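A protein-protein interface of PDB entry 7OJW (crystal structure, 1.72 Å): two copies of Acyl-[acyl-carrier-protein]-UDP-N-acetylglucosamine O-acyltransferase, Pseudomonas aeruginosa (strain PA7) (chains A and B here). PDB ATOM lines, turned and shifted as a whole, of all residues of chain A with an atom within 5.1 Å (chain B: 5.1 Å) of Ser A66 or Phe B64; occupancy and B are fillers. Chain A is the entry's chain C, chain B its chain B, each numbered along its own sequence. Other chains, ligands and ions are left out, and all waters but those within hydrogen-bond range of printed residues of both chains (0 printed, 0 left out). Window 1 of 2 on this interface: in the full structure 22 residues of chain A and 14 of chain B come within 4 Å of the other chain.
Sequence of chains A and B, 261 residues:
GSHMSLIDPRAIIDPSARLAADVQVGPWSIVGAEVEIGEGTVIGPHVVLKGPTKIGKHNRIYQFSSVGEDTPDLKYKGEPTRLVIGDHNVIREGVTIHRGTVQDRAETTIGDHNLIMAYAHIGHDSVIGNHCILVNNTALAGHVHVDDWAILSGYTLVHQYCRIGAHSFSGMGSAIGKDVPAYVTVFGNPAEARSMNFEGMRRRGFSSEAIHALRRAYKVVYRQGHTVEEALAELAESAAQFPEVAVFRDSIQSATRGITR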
ATOM      1  N   HIS A  46     -31.181 -11.256  18.088  1.00  0.00           N
ATOM      2  CA  HIS A  46     -31.451 -12.391  18.986  1.00  0.00           C
ATOM      3  C   HIS A  46     -30.200 -13.032  19.561  1.00  0.00           C
ATOM      4  O   HIS A  46     -30.152 -14.261  19.695  1.00  0.00           O
ATOM      5  CB  HIS A  46     -32.249 -13.499  18.248  1.00  0.00           C
ATOM      6  CG  HIS A  46     -33.544 -13.056  17.663  1.00  0.00           C
ATOM      7  ND1 HIS A  46     -34.563 -12.618  18.451  1.00  0.00           N
ATOM      8  CD2 HIS A  46     -33.945 -13.024  16.377  1.00  0.00           C
ATOM      9  CE1 HIS A  46     -35.571 -12.349  17.627  1.00  0.00           C
ATOM     10  NE2 HIS A  46     -35.248 -12.589  16.382  1.00  0.00           N
ATOM     11  N   VAL A  47     -29.187 -12.234  19.883  1.00  0.00           N
ATOM     12  CA  VAL A  47     -27.971 -12.776  20.499  1.00  0.00           C
ATOM     13  C   VAL A  47     -27.981 -12.452  21.993  1.00  0.00           C
ATOM     14  O   VAL A  47     -28.355 -11.342  22.370  1.00  0.00           O
ATOM     15  CB  VAL A  47     -26.706 -12.198  19.809  1.00  0.00           C
ATOM     16  CG1 VAL A  47     -25.432 -12.576  20.559  1.00  0.00           C
ATOM     17  CG2 VAL A  47     -26.645 -12.626  18.329  1.00  0.00           C
ATOM     18  N   VAL A  48     -27.485 -13.370  22.836  1.00  0.00           N
ATOM     19  CA  VAL A  48     -27.373 -13.097  24.278  1.00  0.00           C
ATOM     20  C   VAL A  48     -25.908 -13.136  24.616  1.00  0.00           C
ATOM     21  O   VAL A  48     -25.263 -14.181  24.448  1.00  0.00           O
ATOM     22  CB  VAL A  48     -28.193 -14.078  25.159  1.00  0.00           C
ATOM     23  CG1 VAL A  48     -27.920 -13.841  26.666  1.00  0.00           C
ATOM     24  CG2 VAL A  48     -29.681 -13.975  24.842  1.00  0.00           C
ATOM     25  N   PHE A  64     -29.353 -16.304  17.979  1.00  0.00           N
ATOM     26  CA  PHE A  64     -29.665 -17.417  18.860  1.00  0.00           C
ATOM     27  C   PHE A  64     -28.458 -18.003  19.591  1.00  0.00           C
ATOM     28  O   PHE A  64     -28.620 -19.024  20.254  1.00  0.00           O
ATOM     29  CB  PHE A  64     -30.462 -18.546  18.143  1.00  0.00           C
ATOM     30  CG  PHE A  64     -31.552 -18.004  17.250  1.00  0.00           C
ATOM     31  CD1 PHE A  64     -32.476 -17.084  17.734  1.00  0.00           C
ATOM     32  CD2 PHE A  64     -31.621 -18.371  15.902  1.00  0.00           C
ATOM     33  CE1 PHE A  64     -33.433 -16.517  16.891  1.00  0.00           C
ATOM     34  CE2 PHE A  64     -32.615 -17.835  15.063  1.00  0.00           C
ATOM     35  CZ  PHE A  64     -33.495 -16.884  15.569  1.00  0.00           C
ATOM     36  N   SER A  65     -27.315 -17.322  19.523  1.00  0.00           N
ATOM     37  CA  SER A  65     -26.090 -17.689  20.250  1.00  0.00           C
ATOM     38  C   SER A  65     -26.200 -17.193  21.681  1.00  0.00           C
ATOM     39  O   SER A  65     -26.810 -16.144  21.941  1.00  0.00           O
ATOM     40  CB  SER A  65     -24.868 -17.058  19.583  1.00  0.00           C
ATOM     41  OG  SER A  65     -24.569 -17.821  18.422  1.00  0.00           O
ATOM     42  N   SER A  66     -25.571 -17.926  22.612  1.00  0.00           N
ATOM     43  CA  SER A  66     -25.488 -17.560  24.043  1.00  0.00           C
ATOM     44  C   SER A  66     -24.007 -17.611  24.369  1.00  0.00           C
ATOM     45  O   SER A  66     -23.417 -18.684  24.477  1.00  0.00           O
ATOM     46  CB  SER A  66     -26.271 -18.540  24.904  1.00  0.00           C
ATOM     47  OG  SER A  66     -27.653 -18.416  24.637  1.00  0.00           O
ATOM     48  N   VAL A  67     -23.390 -16.435  24.422  1.00  0.00           N
ATOM     49  CA  VAL A  67     -21.952 -16.334  24.561  1.00  0.00           C
ATOM     50  C   VAL A  67     -21.641 -15.680  25.911  1.00  0.00           C
ATOM     51  O   VAL A  67     -22.086 -14.560  26.175  1.00  0.00           O
ATOM     52  CB  VAL A  67     -21.392 -15.523  23.354  1.00  0.00           C
ATOM     53  CG1 VAL A  67     -19.895 -15.217  23.512  1.00  0.00           C
ATOM     54  CG2 VAL A  67     -21.664 -16.240  22.022  1.00  0.00           C
ATOM     55  N   GLY A  68     -20.895 -16.389  26.738  1.00  0.00           N
ATOM     56  CA  GLY A  68     -20.466 -15.931  28.058  1.00  0.00           C
ATOM     57  C   GLY A  68     -21.345 -16.444  29.169  1.00  0.00           C
ATOM     58  O   GLY A  68     -21.456 -15.797  30.201  1.00  0.00           O
ATOM     59  N   GLU A  69     -21.954 -17.640  28.985  1.00  0.00           N
ATOM     60  CA  GLU A  69     -22.822 -18.254  29.994  1.00  0.00           C
ATOM     61  C   GLU A  69     -22.028 -18.753  31.169  1.00  0.00           C
ATOM     62  O   GLU A  69     -20.841 -19.027  31.044  1.00  0.00           O
ATOM     63  CB  GLU A  69     -23.579 -19.437  29.384  1.00  0.00           C
ATOM     64  CG  GLU A  69     -24.221 -19.075  28.053  1.00  0.00           C
ATOM     65  CD  GLU A  69     -25.009 -20.237  27.517  1.00  0.00           C
ATOM     66  OE1 GLU A  69     -24.403 -21.090  26.829  1.00  0.00           O
ATOM     67  OE2 GLU A  69     -26.228 -20.300  27.797  1.00  0.00           O
ATOM     68  N   VAL A  95     -24.677 -21.068  18.844  1.00  0.00           N
ATOM     69  CA  VAL A  95     -23.459 -21.497  19.546  1.00  0.00           C
ATOM     70  C   VAL A  95     -23.588 -21.168  21.037  1.00  0.00           C
ATOM     71  O   VAL A  95     -24.124 -20.114  21.380  1.00  0.00           O
ATOM     72  CB  VAL A  95     -22.212 -20.820  18.901  1.00  0.00           C
ATOM     73  CG1 VAL A  95     -20.964 -21.018  19.758  1.00  0.00           C
ATOM     74  CG2 VAL A  95     -21.959 -21.369  17.480  1.00  0.00           C
ATOM     75  N   THR A  96     -23.059 -22.050  21.921  1.00  0.00           N
ATOM     76  CA  THR A  96     -23.023 -21.782  23.369  1.00  0.00           C
ATOM     77  C   THR A  96     -21.583 -21.791  23.816  1.00  0.00           C
ATOM     78  O   THR A  96     -20.838 -22.712  23.477  1.00  0.00           O
ATOM     79  CB  THR A  96     -23.888 -22.772  24.128  1.00  0.00           C
ATOM     80  OG1 THR A  96     -23.480 -24.130  23.812  1.00  0.00           O
ATOM     81  CG2 THR A  96     -25.364 -22.587  23.803  1.00  0.00           C
ATOM     82  N   ILE A  97     -21.164 -20.715  24.517  1.00  0.00           N
ATOM     83  CA  ILE A  97     -19.778 -20.609  24.980  1.00  0.00           C
ATOM     84  C   ILE A  97     -19.852 -20.223  26.439  1.00  0.00           C
ATOM     85  O   ILE A  97     -20.460 -19.208  26.769  1.00  0.00           O
ATOM     86  CB  ILE A  97     -18.941 -19.601  24.161  1.00  0.00           C
ATOM     87  CG1 ILE A  97     -19.055 -19.853  22.623  1.00  0.00           C
ATOM     88  CG2 ILE A  97     -17.459 -19.574  24.657  1.00  0.00           C
ATOM     89  CD1 ILE A  97     -18.271 -18.774  21.796  1.00  0.00           C
ATOM     90  N   PRO B  45     -35.245 -14.509  28.634  1.00  0.00           N
ATOM     91  CA  PRO B  45     -35.760 -13.870  27.409  1.00  0.00           C
ATOM     92  C   PRO B  45     -35.875 -14.874  26.272  1.00  0.00           C
ATOM     93  O   PRO B  45     -35.225 -15.911  26.339  1.00  0.00           O
ATOM     94  CB  PRO B  45     -34.655 -12.851  27.087  1.00  0.00           C
ATOM     95  CG  PRO B  45     -33.371 -13.569  27.532  1.00  0.00           C
ATOM     96  CD  PRO B  45     -33.776 -14.345  28.775  1.00  0.00           C
ATOM     97  N   HIS B  46     -36.643 -14.571  25.193  1.00  0.00           N
ATOM     98  CA  HIS B  46     -36.702 -15.465  24.030  1.00  0.00           C
ATOM     99  C   HIS B  46     -37.152 -16.887  24.342  1.00  0.00           C
ATOM    100  O   HIS B  46     -36.659 -17.830  23.716  1.00  0.00           O
ATOM    101  CB  HIS B  46     -35.342 -15.496  23.323  1.00  0.00           C
ATOM    102  CG  HIS B  46     -34.859 -14.173  22.830  1.00  0.00           C
ATOM    103  ND1 HIS B  46     -35.563 -13.458  21.901  1.00  0.00           N
ATOM    104  CD2 HIS B  46     -33.703 -13.525  23.094  1.00  0.00           C
ATOM    105  CE1 HIS B  46     -34.841 -12.377  21.658  1.00  0.00           C
ATOM    106  NE2 HIS B  46     -33.712 -12.391  22.349  1.00  0.00           N
ATOM    107  N   VAL B  47     -38.039 -17.062  25.327  1.00  0.00           N
ATOM    108  CA  VAL B  47     -38.562 -18.392  25.658  1.00  0.00           C
ATOM    109  C   VAL B  47     -39.946 -18.520  25.073  1.00  0.00           C
ATOM    110  O   VAL B  47     -40.712 -17.560  25.137  1.00  0.00           O
ATOM    111  CB  VAL B  47     -38.586 -18.602  27.196  1.00  0.00           C
ATOM    112  CG1 VAL B  47     -39.229 -19.963  27.578  1.00  0.00           C
ATOM    113  CG2 VAL B  47     -37.176 -18.524  27.746  1.00  0.00           C
ATOM    114  N   TYR B  62     -34.207 -21.077  30.430  1.00  0.00           N
ATOM    115  CA  TYR B  62     -33.331 -20.203  29.664  1.00  0.00           C
ATOM    116  C   TYR B  62     -33.803 -19.979  28.226  1.00  0.00           C
ATOM    117  O   TYR B  62     -34.632 -20.704  27.673  1.00  0.00           O
ATOM    118  CB  TYR B  62     -31.907 -20.757  29.619  1.00  0.00           C
ATOM    119  CG  TYR B  62     -31.151 -20.579  30.922  1.00  0.00           C
ATOM    120  CD1 TYR B  62     -31.479 -21.326  32.053  1.00  0.00           C
ATOM    121  CD2 TYR B  62     -30.120 -19.651  31.028  1.00  0.00           C
ATOM    122  CE1 TYR B  62     -30.789 -21.155  33.261  1.00  0.00           C
ATOM    123  CE2 TYR B  62     -29.446 -19.448  32.234  1.00  0.00           C
ATOM    124  CZ  TYR B  62     -29.775 -20.213  33.342  1.00  0.00           C
ATOM    125  OH  TYR B  62     -29.067 -20.025  34.514  1.00  0.00           O
ATOM    126  N   GLN B  63     -33.212 -18.950  27.637  1.00  0.00           N
ATOM    127  CA  GLN B  63     -33.506 -18.441  26.309  1.00  0.00           C
ATOM    128  C   GLN B  63     -33.505 -19.503  25.209  1.00  0.00           C
ATOM    129  O   GLN B  63     -32.717 -20.453  25.241  1.00  0.00           O
ATOM    130  CB  GLN B  63     -32.489 -17.352  25.940  1.00  0.00           C
ATOM    131  CG  GLN B  63     -31.037 -17.814  25.957  1.00  0.00           C
ATOM    132  CD  GLN B  63     -30.338 -17.597  27.271  1.00  0.00           C
ATOM    133  OE1 GLN B  63     -30.951 -17.249  28.281  1.00  0.00           O
ATOM    134  NE2 GLN B  63     -29.041 -17.799  27.277  1.00  0.00           N
ATOM    135  N   PHE B  64     -34.375 -19.320  24.220  1.00  0.00           N
ATOM    136  CA  PHE B  64     -34.454 -20.132  23.005  1.00  0.00           C
ATOM    137  C   PHE B  64     -35.041 -21.523  23.245  1.00  0.00           C
ATOM    138  O   PHE B  64     -35.059 -22.323  22.315  1.00  0.00           O
ATOM    139  CB  PHE B  64     -33.109 -20.184  22.201  1.00  0.00           C
ATOM    140  CG  PHE B  64     -32.399 -18.845  22.104  1.00  0.00           C
ATOM    141  CD1 PHE B  64     -33.060 -17.710  21.615  1.00  0.00           C
ATOM    142  CD2 PHE B  64     -31.075 -18.708  22.515  1.00  0.00           C
ATOM    143  CE1 PHE B  64     -32.394 -16.473  21.526  1.00  0.00           C
ATOM    144  CE2 PHE B  64     -30.418 -17.474  22.446  1.00  0.00           C
ATOM    145  CZ  PHE B  64     -31.089 -16.355  21.982  1.00  0.00           C
ATOM    146  N   SER B  65     -35.624 -21.748  24.429  1.00  0.00           N
ATOM    147  CA  SER B  65     -36.310 -23.005  24.756  1.00  0.00           C
ATOM    148  C   SER B  65     -37.731 -22.939  24.224  1.00  0.00           C
ATOM    149  O   SER B  65     -38.321 -21.844  24.184  1.00  0.00           O
ATOM    150  CB  SER B  65     -36.328 -23.213  26.271  1.00  0.00           C
ATOM    151  OG  SER B  65     -35.007 -23.518  26.692  1.00  0.00           O
ATOM    152  N   SER B  66     -38.298 -24.107  23.849  1.00  0.00           N
ATOM    153  CA  SER B  66     -39.687 -24.240  23.406  1.00  0.00           C
ATOM    154  C   SER B  66     -40.244 -25.319  24.309  1.00  0.00           C
ATOM    155  O   SER B  66     -39.906 -26.501  24.164  1.00  0.00           O
ATOM    156  CB  SER B  66     -39.787 -24.667  21.945  1.00  0.00           C
ATOM    157  OG  SER B  66     -39.217 -23.657  21.131  1.00  0.00           O
ATOM    158  N   GLU B  93     -30.611 -23.424  27.616  1.00  0.00           N
ATOM    159  CA  GLU B  93     -30.938 -22.835  26.314  1.00  0.00           C
ATOM    160  C   GLU B  93     -31.323 -23.843  25.278  1.00  0.00           C
ATOM    161  O   GLU B  93     -30.718 -24.920  25.213  1.00  0.00           O
ATOM    162  CB  GLU B  93     -29.762 -21.977  25.799  1.00  0.00           C
ATOM    163  CG  GLU B  93     -28.401 -22.640  25.728  1.00  0.00           C
ATOM    164  CD  GLU B  93     -27.568 -22.726  27.001  1.00  0.00           C
ATOM    165  OE1 GLU B  93     -28.104 -22.485  28.106  1.00  0.00           O
ATOM    166  OE2 GLU B  93     -26.366 -23.064  26.893  1.00  0.00           O
ATOM    167  N   GLY B  94     -32.311 -23.502  24.449  1.00  0.00           N
ATOM    168  CA  GLY B  94     -32.663 -24.310  23.284  1.00  0.00           C
ATOM    169  C   GLY B  94     -33.336 -25.653  23.563  1.00  0.00           C
ATOM    170  O   GLY B  94     -33.491 -26.448  22.639  1.00  0.00           O
ATOM    171  N   VAL B  95     -33.725 -25.941  24.835  1.00  0.00           N
ATOM    172  CA  VAL B  95     -34.374 -27.229  25.149  1.00  0.00           C
ATOM    173  C   VAL B  95     -35.736 -27.270  24.528  1.00  0.00           C
ATOM    174  O   VAL B  95     -36.414 -26.251  24.531  1.00  0.00           O
ATOM    175  CB  VAL B  95     -34.410 -27.425  26.686  1.00  0.00           C
ATOM    176  CG1 VAL B  95     -35.291 -28.633  27.098  1.00  0.00           C
ATOM    177  CG2 VAL B  95     -32.985 -27.584  27.195  1.00  0.00           C
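The side-chain amide nitrogen (NE2) of Gln B63 is in hydrogen-bond range of the side-chain hydroxyl (OG) of Ser A66. OE2 of Glu B93 sits close to OE1 of Glu A69 (2.8 Å).
O of Gln B63 sits at hydrogen-bond distance from N of Gly B94 (3.2 Å). O of His B46 lies within hydrogen-bond range of N of Phe B64, 2.8 Å away. The backbone carbonyl oxygen (O) of Val A95 sits at hydrogen-bond distance from the backbone NH (N) of Ser A66 (2.9 Å). The backbone NH of Val A67 lies within hydrogen-bond range of the backbone carbonyl oxygen of Val A48, 2.9 Å away. N of Ile A97 is in hydrogen-bond range of O of Ser A66, at 3.0 Å. The backbone NH (N) of Glu A69 is in hydrogen-bond range of the backbone carbonyl oxygen (O) of Ile A97.
Among the printed residues, merely in contact across the chains: His A46 with His B46, Phe A64 with Phe B64, His A46 with Phe B64, Thr A96 with Glu B93, Ser A66 with Phe B64, Glu A69 with Gln B63, Ser A65 with Phe B64 and Val A48 with Phe B64.
Of chain B, only Gln B63 and Phe B64 come within 4 Å of Ser A66. Phe B64 touches just these residues of chain A: His A46, Val A48, Phe A64, Ser A65 and Ser A66. Of the printed residues of chain B, Phe A64 touches Phe B64 (3.2 Å). Printed residues of chain B within 4 Å of Ser A65: Phe B64 (3.9 Å). Printed residues of chain B within 4 Å of His A46: His B46 (3.2 Å) and Phe B64 (3.2 Å). Of the printed residues of chain B, Glu A69 touches Gln B63 and Glu B93. Of the printed residues of chain B, Thr A96 touches Glu B93 (3.3 Å).
Hydrophobic or aromatic side chains of chain A within 4 Å of the printed part of chain B: His A46, Val A48 and Phe A64. Printed residues of chain B that touch a printed residue of chain A: His B46, Gln B63, Phe B64 and Glu B93. Hydrophobic or aromatic side chains of chain B that line the printed part of chain A: His B46 and Phe B64. Among the printed residues, no Asp or Glu carboxylate lies within 4 Å of a Lys or Arg side-chain nitrogen of the other chain.
His A46 touches its own counterpart, His B46. His A46 touches Phe B64, but with the chains exchanged Phe A64 does not touch His B46 (6.2 Å). Phe B64 touches its own counterpart, Phe A64. Ser A66 touches Phe B64, but with the chains exchanged Phe A64 does not touch Ser B66 (10.0 Å). Positions printed for both chains: 46, 47, 64, 65, 66 and 95. Of the 10 pairs that touch across the chains among the printed residues, 2 have their exchanged pair printed and touching as well.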
